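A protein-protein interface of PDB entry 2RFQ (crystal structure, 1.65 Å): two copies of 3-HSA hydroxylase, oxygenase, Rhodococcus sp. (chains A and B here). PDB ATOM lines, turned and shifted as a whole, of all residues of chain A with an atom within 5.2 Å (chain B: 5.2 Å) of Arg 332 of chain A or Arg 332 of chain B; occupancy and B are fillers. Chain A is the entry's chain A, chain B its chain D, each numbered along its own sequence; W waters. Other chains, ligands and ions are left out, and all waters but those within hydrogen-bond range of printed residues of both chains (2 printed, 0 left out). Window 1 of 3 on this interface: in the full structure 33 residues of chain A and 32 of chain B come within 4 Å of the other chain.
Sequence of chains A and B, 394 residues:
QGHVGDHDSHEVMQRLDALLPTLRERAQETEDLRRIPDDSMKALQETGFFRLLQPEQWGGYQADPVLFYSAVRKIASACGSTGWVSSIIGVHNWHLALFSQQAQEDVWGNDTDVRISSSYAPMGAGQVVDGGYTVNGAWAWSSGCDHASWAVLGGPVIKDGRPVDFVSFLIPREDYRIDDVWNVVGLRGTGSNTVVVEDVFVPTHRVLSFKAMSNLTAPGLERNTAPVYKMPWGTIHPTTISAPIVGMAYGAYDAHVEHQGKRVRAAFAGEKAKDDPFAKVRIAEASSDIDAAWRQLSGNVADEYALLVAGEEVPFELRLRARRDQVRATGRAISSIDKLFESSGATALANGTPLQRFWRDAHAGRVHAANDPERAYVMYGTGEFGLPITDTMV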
ATOM      1  N   SER A 288      16.965   6.030  12.851  1.00  0.00           N
ATOM      2  CA  SER A 288      17.740   6.997  13.638  1.00  0.00           C
ATOM      3  C   SER A 288      16.923   7.542  14.789  1.00  0.00           C
ATOM      4  O   SER A 288      17.422   7.701  15.900  1.00  0.00           O
ATOM      5  CB  SER A 288      18.241   8.135  12.752  1.00  0.00           C
ATOM      6  OG  SER A 288      18.968   9.087  13.530  1.00  0.00           O
ATOM      7  N   ASP A 289      15.664   7.832  14.520  1.00  0.00           N
ATOM      8  CA  ASP A 289      14.800   8.441  15.557  1.00  0.00           C
ATOM      9  C   ASP A 289      14.430   7.451  16.659  1.00  0.00           C
ATOM     10  O   ASP A 289      14.333   7.833  17.836  1.00  0.00           O
ATOM     11  CB  ASP A 289      13.571   9.070  14.925  1.00  0.00           C
ATOM     12  CG  ASP A 289      13.923  10.262  14.045  1.00  0.00           C
ATOM     13  OD1 ASP A 289      15.068  10.784  14.166  1.00  0.00           O
ATOM     14  OD2 ASP A 289      13.050  10.691  13.257  1.00  0.00           O
ATOM     15  N   ILE A 290      14.260   6.188  16.284  1.00  0.00           N
ATOM     16  CA  ILE A 290      14.032   5.126  17.274  1.00  0.00           C
ATOM     17  C   ILE A 290      15.266   5.018  18.154  1.00  0.00           C
ATOM     18  O   ILE A 290      15.152   4.990  19.383  1.00  0.00           O
ATOM     19  CB  ILE A 290      13.699   3.773  16.595  1.00  0.00           C
ATOM     20  CG1 ILE A 290      12.330   3.884  15.900  1.00  0.00           C
ATOM     21  CG2 ILE A 290      13.721   2.660  17.643  1.00  0.00           C
ATOM     22  CD1 ILE A 290      12.119   2.775  14.848  1.00  0.00           C
ATOM     23  N   ALA A 292      17.500   7.310  18.767  1.00  0.00           N
ATOM     24  CA  ALA A 292      17.603   8.506  19.617  1.00  0.00           C
ATOM     25  C   ALA A 292      16.673   8.385  20.833  1.00  0.00           C
ATOM     26  O   ALA A 292      17.056   8.709  21.969  1.00  0.00           O
ATOM     27  CB  ALA A 292      17.272   9.757  18.820  1.00  0.00           C
ATOM     28  N   ALA A 293      15.448   7.927  20.573  1.00  0.00           N
ATOM     29  CA  ALA A 293      14.464   7.698  21.639  1.00  0.00           C
ATOM     30  C   ALA A 293      15.044   6.787  22.708  1.00  0.00           C
ATOM     31  O   ALA A 293      15.007   7.116  23.883  1.00  0.00           O
ATOM     32  CB  ALA A 293      13.191   7.096  21.065  1.00  0.00           C
ATOM     33  N   GLN A 296      18.092   8.363  24.743  1.00  0.00           N
ATOM     34  CA  GLN A 296      17.663   9.304  25.801  1.00  0.00           C
ATOM     35  C   GLN A 296      16.896   8.610  26.924  1.00  0.00           C
ATOM     36  O   GLN A 296      17.145   8.865  28.121  1.00  0.00           O
ATOM     37  CB  GLN A 296      16.817  10.419  25.194  1.00  0.00           C
ATOM     38  CG  GLN A 296      17.644  11.246  24.217  1.00  0.00           C
ATOM     39  CD  GLN A 296      16.930  12.489  23.749  1.00  0.00           C
ATOM     40  OE1 GLN A 296      15.813  12.417  23.211  1.00  0.00           O
ATOM     41  NE2 GLN A 296      17.570  13.656  23.960  1.00  0.00           N
ATOM     42  N   ARG A 328       9.070  12.584  24.756  1.00  0.00           N
ATOM     43  CA  ARG A 328       9.558  12.723  23.377  1.00  0.00           C
ATOM     44  C   ARG A 328       9.913  11.376  22.751  1.00  0.00           C
ATOM     45  O   ARG A 328       9.714  11.196  21.553  1.00  0.00           O
ATOM     46  CB  ARG A 328      10.742  13.681  23.293  1.00  0.00           C
ATOM     47  CG  ARG A 328      10.873  14.297  21.870  1.00  0.00           C
ATOM     48  CD  ARG A 328      11.583  15.681  21.949  1.00  0.00           C
ATOM     49  NE  ARG A 328      11.711  16.398  20.671  1.00  0.00           N
ATOM     50  CZ  ARG A 328      10.710  17.041  20.069  1.00  0.00           C
ATOM     51  NH1 ARG A 328       9.479  17.055  20.606  1.00  0.00           N
ATOM     52  NH2 ARG A 328      10.919  17.685  18.922  1.00  0.00           N
ATOM     53  N   ALA A 329      10.436  10.443  23.553  1.00  0.00           N
ATOM     54  CA  ALA A 329      10.801   9.114  23.060  1.00  0.00           C
ATOM     55  C   ALA A 329       9.550   8.405  22.528  1.00  0.00           C
ATOM     56  O   ALA A 329       9.577   7.795  21.449  1.00  0.00           O
ATOM     57  CB  ALA A 329      11.419   8.305  24.168  1.00  0.00           C
ATOM     58  N   THR A 330       8.445   8.510  23.270  1.00  0.00           N
ATOM     59  CA  THR A 330       7.162   7.978  22.779  1.00  0.00           C
ATOM     60  C   THR A 330       6.812   8.615  21.433  1.00  0.00           C
ATOM     61  O   THR A 330       6.478   7.918  20.479  1.00  0.00           O
ATOM     62  CB  THR A 330       6.050   8.230  23.805  1.00  0.00           C
ATOM     63  OG1 THR A 330       6.314   7.371  24.930  1.00  0.00           O
ATOM     64  CG2 THR A 330       4.650   7.936  23.206  1.00  0.00           C
ATOM     65  N   GLY A 331       6.927   9.935  21.363  1.00  0.00           N
ATOM     66  CA  GLY A 331       6.650  10.664  20.115  1.00  0.00           C
ATOM     67  C   GLY A 331       7.532  10.220  18.959  1.00  0.00           C
ATOM     68  O   GLY A 331       7.030  10.014  17.846  1.00  0.00           O
ATOM     69  N   ARG A 332       8.842  10.070  19.212  1.00  0.00           N
ATOM     70  CA  ARG A 332       9.775   9.629  18.164  1.00  0.00           C
ATOM     71  C   ARG A 332       9.421   8.210  17.685  1.00  0.00           C
ATOM     72  O   ARG A 332       9.484   7.901  16.493  1.00  0.00           O
ATOM     73  CB  ARG A 332      11.212   9.622  18.692  1.00  0.00           C
ATOM     74  CG  ARG A 332      11.776  11.016  19.043  1.00  0.00           C
ATOM     75  CD  ARG A 332      13.284  10.905  19.303  1.00  0.00           C
ATOM     76  NE  ARG A 332      13.729  11.895  20.292  1.00  0.00           N
ATOM     77  CZ  ARG A 332      14.080  13.156  20.018  1.00  0.00           C
ATOM     78  NH1 ARG A 332      14.486  13.960  21.000  1.00  0.00           N
ATOM     79  NH2 ARG A 332      13.988  13.629  18.780  1.00  0.00           N
ATOM     80  N   ALA A 333       9.090   7.343  18.634  1.00  0.00           N
ATOM     81  CA  ALA A 333       8.726   5.958  18.314  1.00  0.00           C
ATOM     82  C   ALA A 333       7.490   5.920  17.415  1.00  0.00           C
ATOM     83  O   ALA A 333       7.478   5.226  16.380  1.00  0.00           O
ATOM     84  CB  ALA A 333       8.529   5.152  19.578  1.00  0.00           C
ATOM     85  N   ILE A 334       6.460   6.671  17.781  1.00  0.00           N
ATOM     86  CA  ILE A 334       5.214   6.687  16.988  1.00  0.00           C
ATOM     87  C   ILE A 334       5.451   7.324  15.613  1.00  0.00           C
ATOM     88  O   ILE A 334       4.985   6.800  14.599  1.00  0.00           O
ATOM     89  CB  ILE A 334       4.094   7.381  17.758  1.00  0.00           C
ATOM     90  CG1 ILE A 334       3.776   6.547  19.007  1.00  0.00           C
ATOM     91  CG2 ILE A 334       2.853   7.504  16.891  1.00  0.00           C
ATOM     92  CD1 ILE A 334       2.946   7.263  20.052  1.00  0.00           C
ATOM     93  N   SER A 335       6.156   8.456  15.571  1.00  0.00           N
ATOM     94  CA  SER A 335       6.473   9.084  14.275  1.00  0.00           C
ATOM     95  C   SER A 335       7.201   8.119  13.344  1.00  0.00           C
ATOM     96  O   SER A 335       6.926   8.064  12.140  1.00  0.00           O
ATOM     97  CB  SER A 335       7.296  10.340  14.515  1.00  0.00           C
ATOM     98  OG  SER A 335       7.676  10.972  13.301  1.00  0.00           O
ATOM     99  N   SER A 336       8.122   7.340  13.914  1.00  0.00           N
ATOM    100  CA  SER A 336       8.900   6.378  13.142  1.00  0.00           C
ATOM    101  C   SER A 336       8.032   5.234  12.631  1.00  0.00           C
ATOM    102  O   SER A 336       8.138   4.847  11.456  1.00  0.00           O
ATOM    103  CB  SER A 336      10.041   5.876  14.006  1.00  0.00           C
ATOM    104  OG  SER A 336      10.876   7.003  14.333  1.00  0.00           O
ATOM    105  N   ILE A 337       7.157   4.708  13.489  1.00  0.00           N
ATOM    106  CA  ILE A 337       6.240   3.631  13.048  1.00  0.00           C
ATOM    107  C   ILE A 337       5.343   4.190  11.930  1.00  0.00           C
ATOM    108  O   ILE A 337       5.095   3.525  10.899  1.00  0.00           O
ATOM    109  CB  ILE A 337       5.374   3.100  14.212  1.00  0.00           C
ATOM    110  CG1 ILE A 337       6.282   2.379  15.211  1.00  0.00           C
ATOM    111  CG2 ILE A 337       4.302   2.120  13.674  1.00  0.00           C
ATOM    112  CD1 ILE A 337       5.633   2.160  16.537  1.00  0.00           C
ATOM    113  N   SER B 288      15.875  18.924  23.850  1.00  0.00           N
ATOM    114  CA  SER B 288      15.861  17.462  23.708  1.00  0.00           C
ATOM    115  C   SER B 288      16.521  17.033  22.403  1.00  0.00           C
ATOM    116  O   SER B 288      17.323  16.084  22.378  1.00  0.00           O
ATOM    117  CB  SER B 288      14.425  16.906  23.791  1.00  0.00           C
ATOM    118  OG  SER B 288      14.452  15.495  23.631  1.00  0.00           O
ATOM    119  N   ASP B 289      16.198  17.738  21.327  1.00  0.00           N
ATOM    120  CA  ASP B 289      16.726  17.376  20.007  1.00  0.00           C
ATOM    121  C   ASP B 289      18.229  17.647  19.881  1.00  0.00           C
ATOM    122  O   ASP B 289      18.966  16.868  19.234  1.00  0.00           O
ATOM    123  CB  ASP B 289      15.918  18.057  18.898  1.00  0.00           C
ATOM    124  CG  ASP B 289      14.471  17.574  18.849  1.00  0.00           C
ATOM    125  OD1 ASP B 289      14.188  16.494  19.429  1.00  0.00           O
ATOM    126  OD2 ASP B 289      13.632  18.241  18.183  1.00  0.00           O
ATOM    127  N   ILE B 290      18.692  18.726  20.499  1.00  0.00           N
ATOM    128  CA  ILE B 290      20.155  18.989  20.532  1.00  0.00           C
ATOM    129  C   ILE B 290      20.853  17.872  21.290  1.00  0.00           C
ATOM    130  O   ILE B 290      21.870  17.311  20.829  1.00  0.00           O
ATOM    131  CB  ILE B 290      20.446  20.350  21.180  1.00  0.00           C
ATOM    132  CG1 ILE B 290      19.840  21.441  20.294  1.00  0.00           C
ATOM    133  CG2 ILE B 290      21.947  20.541  21.367  1.00  0.00           C
ATOM    134  CD1 ILE B 290      19.744  22.811  21.043  1.00  0.00           C
ATOM    135  N   ALA B 292      19.805  14.786  21.730  1.00  0.00           N
ATOM    136  CA  ALA B 292      19.748  13.580  20.895  1.00  0.00           C
ATOM    137  C   ALA B 292      20.840  13.598  19.829  1.00  0.00           C
ATOM    138  O   ALA B 292      21.520  12.587  19.609  1.00  0.00           O
ATOM    139  CB  ALA B 292      18.376  13.447  20.242  1.00  0.00           C
ATOM    140  N   ALA B 293      21.001  14.744  19.168  1.00  0.00           N
ATOM    141  CA  ALA B 293      22.045  14.891  18.152  1.00  0.00           C
ATOM    142  C   ALA B 293      23.416  14.596  18.749  1.00  0.00           C
ATOM    143  O   ALA B 293      24.215  13.853  18.177  1.00  0.00           O
ATOM    144  CB  ALA B 293      22.018  16.323  17.609  1.00  0.00           C
ATOM    145  N   GLN B 296      23.956  10.753  19.721  1.00  0.00           N
ATOM    146  CA  GLN B 296      24.225   9.881  18.570  1.00  0.00           C
ATOM    147  C   GLN B 296      25.576  10.201  17.941  1.00  0.00           C
ATOM    148  O   GLN B 296      26.358   9.278  17.648  1.00  0.00           O
ATOM    149  CB  GLN B 296      23.120  10.002  17.531  1.00  0.00           C
ATOM    150  CG  GLN B 296      21.786   9.481  18.074  1.00  0.00           C
ATOM    151  CD  GLN B 296      20.734   9.403  17.004  1.00  0.00           C
ATOM    152  OE1 GLN B 296      20.439  10.401  16.336  1.00  0.00           O
ATOM    153  NE2 GLN B 296      20.148   8.220  16.838  1.00  0.00           N
ATOM    154  N   ARG B 328      21.934  13.533  10.393  1.00  0.00           N
ATOM    155  CA  ARG B 328      20.712  13.836  11.155  1.00  0.00           C
ATOM    156  C   ARG B 328      21.009  14.751  12.343  1.00  0.00           C
ATOM    157  O   ARG B 328      20.165  15.592  12.701  1.00  0.00           O
ATOM    158  CB  ARG B 328      20.018  12.558  11.626  1.00  0.00           C
ATOM    159  CG  ARG B 328      18.502  12.802  11.941  1.00  0.00           C
ATOM    160  CD  ARG B 328      17.682  11.526  11.664  1.00  0.00           C
ATOM    161  NE  ARG B 328      16.235  11.705  11.849  1.00  0.00           N
ATOM    162  CZ  ARG B 328      15.435  12.249  10.936  1.00  0.00           C
ATOM    163  NH1 ARG B 328      15.931  12.738   9.780  1.00  0.00           N
ATOM    164  NH2 ARG B 328      14.126  12.315  11.173  1.00  0.00           N
ATOM    165  N   ALA B 329      22.190  14.602  12.941  1.00  0.00           N
ATOM    166  CA  ALA B 329      22.598  15.488  14.041  1.00  0.00           C
ATOM    167  C   ALA B 329      22.662  16.942  13.572  1.00  0.00           C
ATOM    168  O   ALA B 329      22.186  17.852  14.260  1.00  0.00           O
ATOM    169  CB  ALA B 329      23.949  15.048  14.597  1.00  0.00           C
ATOM    170  N   THR B 330      23.258  17.159  12.397  1.00  0.00           N
ATOM    171  CA  THR B 330      23.281  18.502  11.814  1.00  0.00           C
ATOM    172  C   THR B 330      21.846  19.011  11.629  1.00  0.00           C
ATOM    173  O   THR B 330      21.500  20.144  12.003  1.00  0.00           O
ATOM    174  CB  THR B 330      24.017  18.488  10.498  1.00  0.00           C
ATOM    175  OG1 THR B 330      25.405  18.291  10.787  1.00  0.00           O
ATOM    176  CG2 THR B 330      23.783  19.798   9.715  1.00  0.00           C
ATOM    177  N   GLY B 331      20.989  18.151  11.087  1.00  0.00           N
ATOM    178  CA  GLY B 331      19.580  18.518  10.896  1.00  0.00           C
ATOM    179  C   GLY B 331      18.854  18.877  12.193  1.00  0.00           C
ATOM    180  O   GLY B 331      18.119  19.872  12.244  1.00  0.00           O
ATOM    181  N   ARG B 332      19.036  18.055  13.238  1.00  0.00           N
ATOM    182  CA  ARG B 332      18.390  18.305  14.537  1.00  0.00           C
ATOM    183  C   ARG B 332      18.891  19.633  15.134  1.00  0.00           C
ATOM    184  O   ARG B 332      18.122  20.427  15.701  1.00  0.00           O
ATOM    185  CB  ARG B 332      18.723  17.184  15.511  1.00  0.00           C
ATOM    186  CG  ARG B 332      18.178  15.819  15.132  1.00  0.00           C
ATOM    187  CD  ARG B 332      18.395  14.846  16.315  1.00  0.00           C
ATOM    188  NE  ARG B 332      18.536  13.454  15.863  1.00  0.00           N
ATOM    189  CZ  ARG B 332      17.524  12.602  15.631  1.00  0.00           C
ATOM    190  NH1 ARG B 332      17.794  11.358  15.216  1.00  0.00           N
ATOM    191  NH2 ARG B 332      16.244  12.985  15.773  1.00  0.00           N
ATOM    192  N   ALA B 333      20.198  19.877  14.998  1.00  0.00           N
ATOM    193  CA  ALA B 333      20.798  21.104  15.521  1.00  0.00           C
ATOM    194  C   ALA B 333      20.200  22.322  14.831  1.00  0.00           C
ATOM    195  O   ALA B 333      19.820  23.294  15.504  1.00  0.00           O
ATOM    196  CB  ALA B 333      22.323  21.067  15.373  1.00  0.00           C
ATOM    197  N   ILE B 334      20.084  22.270  13.507  1.00  0.00           N
ATOM    198  CA  ILE B 334      19.552  23.407  12.745  1.00  0.00           C
ATOM    199  C   ILE B 334      18.077  23.610  13.055  1.00  0.00           C
ATOM    200  O   ILE B 334      17.619  24.746  13.285  1.00  0.00           O
ATOM    201  CB  ILE B 334      19.806  23.231  11.249  1.00  0.00           C
ATOM    202  CG1 ILE B 334      21.310  23.269  10.996  1.00  0.00           C
ATOM    203  CG2 ILE B 334      19.088  24.333  10.448  1.00  0.00           C
ATOM    204  CD1 ILE B 334      21.738  22.741   9.637  1.00  0.00           C
ATOM    205  N   SER B 335      17.326  22.512  13.082  1.00  0.00           N
ATOM    206  CA  SER B 335      15.900  22.606  13.414  1.00  0.00           C
ATOM    207  C   SER B 335      15.687  23.227  14.794  1.00  0.00           C
ATOM    208  O   SER B 335      14.770  24.066  14.985  1.00  0.00           O
ATOM    209  CB  SER B 335      15.275  21.219  13.367  1.00  0.00           C
ATOM    210  OG  SER B 335      13.888  21.321  13.639  1.00  0.00           O
ATOM    211  N   SER B 336      16.534  22.847  15.746  1.00  0.00           N
ATOM    212  CA  SER B 336      16.437  23.379  17.109  1.00  0.00           C
ATOM    213  C   SER B 336      16.775  24.874  17.133  1.00  0.00           C
ATOM    214  O   SER B 336      16.079  25.662  17.794  1.00  0.00           O
ATOM    215  CB  SER B 336      17.323  22.578  18.060  1.00  0.00           C
ATOM    216  OG  SER B 336      16.915  21.193  18.030  1.00  0.00           O
ATOM    217  N   ILE B 337      17.837  25.266  16.428  1.00  0.00           N
ATOM    218  CA  ILE B 337      18.190  26.691  16.354  1.00  0.00           C
ATOM    219  C   ILE B 337      17.044  27.499  15.722  1.00  0.00           C
ATOM    220  O   ILE B 337      16.662  28.583  16.211  1.00  0.00           O
ATOM    221  CB  ILE B 337      19.485  26.913  15.588  1.00  0.00           C
ATOM    222  CG1 ILE B 337      20.657  26.327  16.383  1.00  0.00           C
ATOM    223  CG2 ILE B 337      19.680  28.445  15.356  1.00  0.00           C
ATOM    224  CD1 ILE B 337      21.986  26.222  15.585  1.00  0.00           C
HETATM  225  O   HOH W   1      14.704  15.428  16.171  1.00  0.00           O
HETATM  226  O   HOH W   2      13.001  12.790  16.098  1.00  0.00           O
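NE2 of Gln 296 of chain A is in hydrogen-bond range of O of Ser 288 of chain B.
The guanidinium group (NH2) of Arg 332 of chain A is in salt-bridge range of the side-chain carboxylate (OD1) of Asp 289 of chain B (2.9 Å).
The guanidinium group (NH1) of Arg 332 of chain A lies within hydrogen-bond range of the side-chain hydroxyl (OG) of Ser 288 of chain B.
The backbone carbonyl oxygen of Ser 288 of chain A lies within hydrogen-bond range of the side-chain amide nitrogen of Gln 296 of chain B, 2.9 Å away.
NE2 of Gln 296 of chain A sits close to N of Ala 292 of chain B.
The side-chain carboxylate (OD1) of Asp 289 of chain A lies within salt-bridge range of the guanidinium group (NH2) of Arg 332 of chain B (3.0 Å).
NE of Arg 328 of chain A lies within salt-bridge range of OD1 of Asp 289 of chain B, at 2.8 Å.
NH1 of Arg 332 of chain B sits at hydrogen-bond distance from OG of Ser 288 of chain A (3.1 Å).
NE2 of Gln 296 of chain B lies close to N of Ala 292 of chain A (3.4 Å).
OD1 of Asp 289 of chain A lies within salt-bridge range of NE of Arg 328 of chain B, at 2.8 Å.
The backbone carbonyl oxygen of Arg 332 of chain A sits at hydrogen-bond distance from the side-chain hydroxyl of Ser 336 of chain A, at 2.7 Å.
The side-chain hydroxyl (OG) of Ser 336 of chain B is in hydrogen-bond range of the backbone carbonyl oxygen (O) of Arg 332 of chain B, 2.7 Å away.
The side-chain amide oxygen (OE1) of Gln 296 of chain B sits at hydrogen-bond distance from the guanidinium group (NH1) of Arg 332 of chain B, 3.0 Å away.
The side-chain amide oxygen (OE1) of Gln 296 of chain A lies within hydrogen-bond range of the guanidinium group (NH1) of Arg 332 of chain A.
Ser 288 of chain A touches Arg 328 of chain B (OG to CD, 3.3 Å).
CB of Ala 292 of chain A touches NH1 of Arg 332 of chain B (3.98 Å).
Arg 328 of chain A touches Ser 288 of chain B (CD to OG, 3.3 Å).
NH1 of Arg 332 of chain A touches CB of Ala 292 of chain B (3.996 Å).
Arg 332 of chain A touches Arg 332 of chain B.
Printed residues of chain B within 4 Å of Arg 328 of chain A: Ser 288 (3.3 Å) and Asp 289 (2.8 Å).
Of the printed residues of chain B, Arg 332 of chain A touches Ser 288, Asp 289, Ala 292 and Arg 332.
Ile 334 of chain A touches none of the printed residues of chain B.
Of the printed residues of chain A, Ser 288 of chain B touches Gln 296, Arg 328 and Arg 332.
Of the printed residues of chain A, Asp 289 of chain B touches Arg 328 (2.8 Å) and Arg 332 (2.9 Å).
Thr 330 of chain B touches none of the printed residues of chain A.
Arg 332 of chain B touches four residues of chain A.
Of the 16 printed residues of chain B, 6 touch a printed residue of chain A.
Hydrophobic or aromatic side chains of chain B that line the printed part of chain A: Ala 292.
Ser 288 of chain A touches Arg 328 of chain B, and with the chains exchanged Arg 328 of chain A touches Ser 288 of chain B.
Asp 289 of chain A touches Arg 332 of chain B, and with the chains exchanged Arg 332 of chain A touches Asp 289 of chain B.
Ala 292 of chain A touches Gln 296 of chain B, and with the chains exchanged Gln 296 of chain A touches Ala 292 of chain B.
Ala 292 of chain A touches Arg 332 of chain B, and with the chains exchanged Arg 332 of chain A touches Ala 292 of chain B.
Positions printed for both chains: 288, 289, 290, 292, 293, 296, 328, 329, 330, 331, 332, 333, 334, 335, 336 and 337.
Water W1 lies within hydrogen-bond range of the guanidinium group of Arg 332 of chain B (2.9 Å), the guanidinium group of Arg 332 of chain A (3.2 Å) and the side-chain carboxylate of Asp 289 of chain B (3.5 Å).
Water W2 lies within hydrogen-bond range of the guanidinium group of Arg 332 of chain A (3.0 Å), the guanidinium group of Arg 332 of chain B (3.3 Å) and the side-chain carboxylate of Asp 289 of chain A (3.5 Å).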
